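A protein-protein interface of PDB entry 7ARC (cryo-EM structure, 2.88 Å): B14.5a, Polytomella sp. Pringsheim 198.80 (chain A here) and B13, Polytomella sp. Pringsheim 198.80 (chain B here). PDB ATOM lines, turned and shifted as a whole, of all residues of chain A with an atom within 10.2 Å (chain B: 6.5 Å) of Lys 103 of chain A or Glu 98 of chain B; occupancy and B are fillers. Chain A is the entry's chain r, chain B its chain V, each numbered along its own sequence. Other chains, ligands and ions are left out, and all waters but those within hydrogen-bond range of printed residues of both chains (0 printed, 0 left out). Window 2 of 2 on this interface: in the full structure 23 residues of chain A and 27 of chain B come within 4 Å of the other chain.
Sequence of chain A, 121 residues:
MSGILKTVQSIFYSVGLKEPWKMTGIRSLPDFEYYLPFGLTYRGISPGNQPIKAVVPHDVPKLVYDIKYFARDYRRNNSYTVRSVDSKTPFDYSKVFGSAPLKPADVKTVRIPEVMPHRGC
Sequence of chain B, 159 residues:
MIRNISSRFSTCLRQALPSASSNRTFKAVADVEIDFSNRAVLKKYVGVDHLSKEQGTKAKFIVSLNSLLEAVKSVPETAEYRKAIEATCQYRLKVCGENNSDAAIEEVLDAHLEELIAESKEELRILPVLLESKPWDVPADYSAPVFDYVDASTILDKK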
ATOM      1  N   PHE A  97      15.889 -14.157  31.866  1.00  0.00           N
ATOM      2  CA  PHE A  97      15.146 -13.637  30.724  1.00  0.00           C
ATOM      3  C   PHE A  97      15.985 -13.358  29.483  1.00  0.00           C
ATOM      4  O   PHE A  97      15.409 -13.106  28.420  1.00  0.00           O
ATOM      5  CB  PHE A  97      14.407 -12.354  31.130  1.00  0.00           C
ATOM      6  CG  PHE A  97      13.288 -12.589  32.101  1.00  0.00           C
ATOM      7  CD1 PHE A  97      12.308 -13.528  31.832  1.00  0.00           C
ATOM      8  CD2 PHE A  97      13.230 -11.891  33.295  1.00  0.00           C
ATOM      9  CE1 PHE A  97      11.279 -13.752  32.725  1.00  0.00           C
ATOM     10  CE2 PHE A  97      12.205 -12.114  34.193  1.00  0.00           C
ATOM     11  CZ  PHE A  97      11.229 -13.045  33.907  1.00  0.00           C
ATOM     12  N   GLY A  98      17.314 -13.379  29.580  1.00  0.00           N
ATOM     13  CA  GLY A  98      18.136 -13.259  28.387  1.00  0.00           C
ATOM     14  C   GLY A  98      18.024 -14.467  27.479  1.00  0.00           C
ATOM     15  O   GLY A  98      18.073 -14.342  26.253  1.00  0.00           O
ATOM     16  N   SER A  99      17.881 -15.651  28.067  1.00  0.00           N
ATOM     17  CA  SER A  99      17.696 -16.886  27.319  1.00  0.00           C
ATOM     18  C   SER A  99      16.238 -17.164  26.980  1.00  0.00           C
ATOM     19  O   SER A  99      15.953 -18.159  26.308  1.00  0.00           O
ATOM     20  CB  SER A  99      18.275 -18.066  28.106  1.00  0.00           C
ATOM     21  OG  SER A  99      17.548 -18.286  29.302  1.00  0.00           O
ATOM     22  N   ALA A 100      15.314 -16.321  27.430  1.00  0.00           N
ATOM     23  CA  ALA A 100      13.906 -16.536  27.129  1.00  0.00           C
ATOM     24  C   ALA A 100      13.602 -16.146  25.683  1.00  0.00           C
ATOM     25  O   ALA A 100      14.108 -15.132  25.193  1.00  0.00           O
ATOM     26  CB  ALA A 100      13.026 -15.730  28.080  1.00  0.00           C
ATOM     27  N   PRO A 101      12.792 -16.938  24.983  1.00  0.00           N
ATOM     28  CA  PRO A 101      12.429 -16.596  23.602  1.00  0.00           C
ATOM     29  C   PRO A 101      11.628 -15.305  23.529  1.00  0.00           C
ATOM     30  O   PRO A 101      10.823 -14.999  24.410  1.00  0.00           O
ATOM     31  CB  PRO A 101      11.593 -17.798  23.148  1.00  0.00           C
ATOM     32  CG  PRO A 101      11.113 -18.430  24.414  1.00  0.00           C
ATOM     33  CD  PRO A 101      12.217 -18.227  25.400  1.00  0.00           C
ATOM     34  N   LEU A 102      11.862 -14.541  22.460  1.00  0.00           N
ATOM     35  CA  LEU A 102      11.066 -13.359  22.160  1.00  0.00           C
ATOM     36  C   LEU A 102      10.102 -13.569  21.003  1.00  0.00           C
ATOM     37  O   LEU A 102       9.230 -12.720  20.785  1.00  0.00           O
ATOM     38  CB  LEU A 102      11.976 -12.163  21.835  1.00  0.00           C
ATOM     39  CG  LEU A 102      12.570 -11.329  22.973  1.00  0.00           C
ATOM     40  CD1 LEU A 102      11.470 -10.638  23.768  1.00  0.00           C
ATOM     41  CD2 LEU A 102      13.468 -12.153  23.884  1.00  0.00           C
ATOM     42  N   LYS A 103      10.233 -14.662  20.264  1.00  0.00           N
ATOM     43  CA  LYS A 103       9.411 -14.968  19.105  1.00  0.00           C
ATOM     44  C   LYS A 103       9.132 -16.461  19.109  1.00  0.00           C
ATOM     45  O   LYS A 103       9.831 -17.223  19.785  1.00  0.00           O
ATOM     46  CB  LYS A 103      10.113 -14.566  17.800  1.00  0.00           C
ATOM     47  CG  LYS A 103      10.321 -13.074  17.620  1.00  0.00           C
ATOM     48  CD  LYS A 103      11.005 -12.783  16.292  1.00  0.00           C
ATOM     49  CE  LYS A 103      11.143 -11.293  16.054  1.00  0.00           C
ATOM     50  NZ  LYS A 103      12.081 -10.671  17.026  1.00  0.00           N
ATOM     51  N   PRO A 104       8.105 -16.913  18.379  1.00  0.00           N
ATOM     52  CA  PRO A 104       7.812 -18.356  18.372  1.00  0.00           C
ATOM     53  C   PRO A 104       8.964 -19.194  17.852  1.00  0.00           C
ATOM     54  O   PRO A 104       9.140 -20.333  18.302  1.00  0.00           O
ATOM     55  CB  PRO A 104       6.570 -18.466  17.475  1.00  0.00           C
ATOM     56  CG  PRO A 104       6.519 -17.199  16.706  1.00  0.00           C
ATOM     57  CD  PRO A 104       7.133 -16.153  17.576  1.00  0.00           C
ATOM     58  N   ALA A 105       9.745 -18.668  16.904  1.00  0.00           N
ATOM     59  CA  ALA A 105      10.821 -19.451  16.305  1.00  0.00           C
ATOM     60  C   ALA A 105      11.883 -19.814  17.336  1.00  0.00           C
ATOM     61  O   ALA A 105      12.427 -20.924  17.314  1.00  0.00           O
ATOM     62  CB  ALA A 105      11.442 -18.682  15.140  1.00  0.00           C
ATOM     63  N   ASP A 106      12.190 -18.893  18.247  1.00  0.00           N
ATOM     64  CA  ASP A 106      13.274 -19.081  19.202  1.00  0.00           C
ATOM     65  C   ASP A 106      12.906 -20.027  20.336  1.00  0.00           C
ATOM     66  O   ASP A 106      13.750 -20.292  21.198  1.00  0.00           O
ATOM     67  CB  ASP A 106      13.694 -17.731  19.790  1.00  0.00           C
ATOM     68  CG  ASP A 106      14.375 -16.836  18.775  1.00  0.00           C
ATOM     69  OD1 ASP A 106      15.014 -17.365  17.842  1.00  0.00           O
ATOM     70  OD2 ASP A 106      14.267 -15.599  18.908  1.00  0.00           O
ATOM     71  N   VAL A 107      11.676 -20.537  20.355  1.00  0.00           N
ATOM     72  CA  VAL A 107      11.232 -21.401  21.440  1.00  0.00           C
ATOM     73  C   VAL A 107      12.013 -22.707  21.415  1.00  0.00           C
ATOM     74  O   VAL A 107      12.116 -23.372  20.376  1.00  0.00           O
ATOM     75  CB  VAL A 107       9.720 -21.654  21.340  1.00  0.00           C
ATOM     76  CG1 VAL A 107       9.297 -22.735  22.320  1.00  0.00           C
ATOM     77  CG2 VAL A 107       8.952 -20.367  21.603  1.00  0.00           C
ATOM     78  N   LYS A 108      12.563 -23.081  22.566  1.00  0.00           N
ATOM     79  CA  LYS A 108      13.260 -24.344  22.742  1.00  0.00           C
ATOM     80  C   LYS A 108      12.516 -25.155  23.788  1.00  0.00           C
ATOM     81  O   LYS A 108      11.993 -24.602  24.760  1.00  0.00           O
ATOM     82  CB  LYS A 108      14.716 -24.136  23.170  1.00  0.00           C
ATOM     83  CG  LYS A 108      15.606 -23.521  22.102  1.00  0.00           C
ATOM     84  CD  LYS A 108      17.013 -23.277  22.625  1.00  0.00           C
ATOM     85  CE  LYS A 108      17.766 -24.581  22.836  1.00  0.00           C
ATOM     86  NZ  LYS A 108      18.062 -25.274  21.553  1.00  0.00           N
ATOM     87  N   LYS B  58      -4.964  -8.523  22.800  1.00  0.00           N
ATOM     88  CA  LYS B  58      -3.610  -8.063  23.094  1.00  0.00           C
ATOM     89  C   LYS B  58      -3.617  -6.763  23.892  1.00  0.00           C
ATOM     90  O   LYS B  58      -2.825  -6.596  24.828  1.00  0.00           O
ATOM     91  CB  LYS B  58      -2.834  -7.882  21.791  1.00  0.00           C
ATOM     92  CG  LYS B  58      -1.380  -7.503  21.972  1.00  0.00           C
ATOM     93  CD  LYS B  58      -0.677  -7.427  20.630  1.00  0.00           C
ATOM     94  CE  LYS B  58       0.777  -7.037  20.794  1.00  0.00           C
ATOM     95  NZ  LYS B  58       1.478  -6.958  19.484  1.00  0.00           N
ATOM     96  N   LEU B  93       6.165  -7.236  27.881  1.00  0.00           N
ATOM     97  CA  LEU B  93       5.880  -6.137  26.966  1.00  0.00           C
ATOM     98  C   LEU B  93       6.731  -6.245  25.707  1.00  0.00           C
ATOM     99  O   LEU B  93       6.260  -5.944  24.604  1.00  0.00           O
ATOM    100  CB  LEU B  93       6.115  -4.799  27.667  1.00  0.00           C
ATOM    101  CG  LEU B  93       4.946  -4.247  28.486  1.00  0.00           C
ATOM    102  CD1 LEU B  93       5.217  -2.821  28.915  1.00  0.00           C
ATOM    103  CD2 LEU B  93       3.655  -4.326  27.695  1.00  0.00           C
ATOM    104  N   LYS B  94       7.980  -6.696  25.846  1.00  0.00           N
ATOM    105  CA  LYS B  94       8.788  -6.987  24.667  1.00  0.00           C
ATOM    106  C   LYS B  94       8.147  -8.088  23.833  1.00  0.00           C
ATOM    107  O   LYS B  94       7.965  -7.933  22.622  1.00  0.00           O
ATOM    108  CB  LYS B  94      10.208  -7.381  25.073  1.00  0.00           C
ATOM    109  CG  LYS B  94      11.018  -6.265  25.705  1.00  0.00           C
ATOM    110  CD  LYS B  94      12.462  -6.690  25.928  1.00  0.00           C
ATOM    111  CE  LYS B  94      12.571  -7.663  27.091  1.00  0.00           C
ATOM    112  NZ  LYS B  94      13.980  -8.018  27.410  1.00  0.00           N
ATOM    113  N   VAL B  95       7.767  -9.197  24.473  1.00  0.00           N
ATOM    114  CA  VAL B  95       7.177 -10.315  23.735  1.00  0.00           C
ATOM    115  C   VAL B  95       5.924  -9.866  22.993  1.00  0.00           C
ATOM    116  O   VAL B  95       5.646 -10.321  21.877  1.00  0.00           O
ATOM    117  CB  VAL B  95       6.884 -11.492  24.684  1.00  0.00           C
ATOM    118  CG1 VAL B  95       6.173 -12.609  23.944  1.00  0.00           C
ATOM    119  CG2 VAL B  95       8.170 -12.017  25.283  1.00  0.00           C
ATOM    120  N   CYS B  96       5.156  -8.956  23.595  1.00  0.00           N
ATOM    121  CA  CYS B  96       4.066  -8.311  22.870  1.00  0.00           C
ATOM    122  C   CYS B  96       4.581  -7.469  21.711  1.00  0.00           C
ATOM    123  O   CYS B  96       3.917  -7.373  20.673  1.00  0.00           O
ATOM    124  CB  CYS B  96       3.229  -7.454  23.816  1.00  0.00           C
ATOM    125  SG  CYS B  96       2.343  -8.388  25.073  1.00  0.00           S
ATOM    126  N   GLY B  97       5.748  -6.847  21.866  1.00  0.00           N
ATOM    127  CA  GLY B  97       6.271  -5.968  20.836  1.00  0.00           C
ATOM    128  C   GLY B  97       6.539  -6.618  19.491  1.00  0.00           C
ATOM    129  O   GLY B  97       5.929  -6.227  18.492  1.00  0.00           O
ATOM    130  N   GLU B  98       7.442  -7.601  19.439  1.00  0.00           N
ATOM    131  CA  GLU B  98       7.783  -8.209  18.153  1.00  0.00           C
ATOM    132  C   GLU B  98       6.617  -9.001  17.571  1.00  0.00           C
ATOM    133  O   GLU B  98       6.429  -9.024  16.348  1.00  0.00           O
ATOM    134  CB  GLU B  98       9.024  -9.099  18.266  1.00  0.00           C
ATOM    135  CG  GLU B  98      10.324  -8.360  18.553  1.00  0.00           C
ATOM    136  CD  GLU B  98      10.534  -8.073  20.018  1.00  0.00           C
ATOM    137  OE1 GLU B  98       9.700  -8.517  20.824  1.00  0.00           O
ATOM    138  OE2 GLU B  98      11.531  -7.403  20.363  1.00  0.00           O
ATOM    139  N   ASN B  99       5.826  -9.655  18.415  1.00  0.00           N
ATOM    140  CA  ASN B  99       4.746 -10.517  17.947  1.00  0.00           C
ATOM    141  C   ASN B  99       3.490  -9.684  17.719  1.00  0.00           C
ATOM    142  O   ASN B  99       2.866  -9.211  18.674  1.00  0.00           O
ATOM    143  CB  ASN B  99       4.482 -11.629  18.956  1.00  0.00           C
ATOM    144  CG  ASN B  99       5.721 -12.437  19.267  1.00  0.00           C
ATOM    145  OD1 ASN B  99       6.026 -13.411  18.584  1.00  0.00           O
ATOM    146  ND2 ASN B  99       6.446 -12.034  20.303  1.00  0.00           N
ATOM    147  N   ASN B 100       3.120  -9.508  16.449  1.00  0.00           N
ATOM    148  CA  ASN B 100       1.888  -8.812  16.098  1.00  0.00           C
ATOM    149  C   ASN B 100       0.658  -9.704  16.195  1.00  0.00           C
ATOM    150  O   ASN B 100      -0.453  -9.188  16.360  1.00  0.00           O
ATOM    151  CB  ASN B 100       1.990  -8.248  14.678  1.00  0.00           C
ATOM    152  CG  ASN B 100       3.075  -7.200  14.541  1.00  0.00           C
ATOM    153  OD1 ASN B 100       4.059  -7.400  13.830  1.00  0.00           O
ATOM    154  ND2 ASN B 100       2.899  -6.074  15.222  1.00  0.00           N
ATOM    155  N   SER B 101       0.828 -11.020  16.091  1.00  0.00           N
ATOM    156  CA  SER B 101      -0.281 -11.953  16.232  1.00  0.00           C
ATOM    157  C   SER B 101      -0.547 -12.257  17.699  1.00  0.00           C
ATOM    158  O   SER B 101       0.384 -12.522  18.465  1.00  0.00           O
ATOM    159  CB  SER B 101       0.018 -13.246  15.475  1.00  0.00           C
ATOM    160  OG  SER B 101      -1.026 -14.188  15.639  1.00  0.00           O
ATOM    161  N   ALA B 104       0.548 -15.740  18.462  1.00  0.00           N
ATOM    162  CA  ALA B 104       1.991 -15.882  18.616  1.00  0.00           C
ATOM    163  C   ALA B 104       2.418 -15.587  20.047  1.00  0.00           C
ATOM    164  O   ALA B 104       3.275 -16.283  20.602  1.00  0.00           O
ATOM    165  CB  ALA B 104       2.718 -14.964  17.636  1.00  0.00           C
ATOM    166  N   VAL B 108       4.531 -18.097  22.508  1.00  0.00           N
ATOM    167  CA  VAL B 108       5.776 -17.744  23.189  1.00  0.00           C
ATOM    168  C   VAL B 108       5.621 -17.857  24.700  1.00  0.00           C
ATOM    169  O   VAL B 108       6.521 -18.346  25.394  1.00  0.00           O
ATOM    170  CB  VAL B 108       6.250 -16.339  22.778  1.00  0.00           C
ATOM    171  CG1 VAL B 108       7.648 -16.094  23.303  1.00  0.00           C
ATOM    172  CG2 VAL B 108       6.254 -16.205  21.275  1.00  0.00           C
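The backbone carbonyl oxygen (O) of Leu 102 of chain A sits at hydrogen-bond distance from the side-chain amide nitrogen (ND2) of Asn 99 of chain B (2.9 Å).
Of the 12 printed residues of chain B, 5 touch a printed residue of chain A. Along chain B the printed residues that touch a printed residue of chain A span positions 94 to 108. Printed residues of chain A that touch a printed residue of chain B: Pro 101, Leu 102, Lys 103 and Pro 104. Among the printed residues, no Asp or Glu carboxylate lies within 4 Å of a Lys or Arg side-chain nitrogen of the other chain.
Among the printed residues, merely in contact across the chains: Pro 104 of chain A with Asn 99 of chain B (3.1 Å), Lys 103 of chain A with Glu 98 of chain B (3.3 Å), Pro 104 of chain A with Val 108 of chain B (3.5 Å), Pro 101 of chain A with Val 108 of chain B (3.5 Å), Lys 103 of chain A with Val 108 of chain B (3.6 Å), Leu 102 of chain A with Lys 94 of chain B (3.7 Å), Lys 103 of chain A with Asn 99 of chain B (3.8 Å) and Leu 102 of chain A with Val 95 of chain B (3.9 Å).
The side-chain amino group (NZ) of Lys 58 of chain B lies within hydrogen-bond range of the backbone carbonyl oxygen (O) of Asn 99 of chain B. OE1 of Glu 98 of chain B lies close to O of Lys 94 of chain B (2.6 Å). The backbone carbonyl oxygen (O) of Val 95 of chain B sits at hydrogen-bond distance from the side-chain amide nitrogen (ND2) of Asn 99 of chain B (2.5 Å).
Of chain B, only Glu 98 (3.3 Å), Asn 99 (3.8 Å) and Val 108 (3.6 Å) come within 4 Å of Lys 103 of chain A. Glu 98 of chain B touches just one residue of chain A: Lys 103 (3.3 Å). Val 95 of chain B touches just one residue of chain A: Leu 102. Gly 97 of chain B touches none of the printed residues of chain A. Of the printed residues of chain B, Pro 104 of chain A touches Asn 99 (3.1 Å) and Val 108 (3.5 Å). Printed residues of chain A within 4 Å of Lys 94 of chain B: Leu 102 (3.7 Å). Cys 96 of chain B touches none of the printed residues of chain A. The nearest residue of chain B that does not touch Lys 103 of chain A is Val 95 of chain B (5.9 Å).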
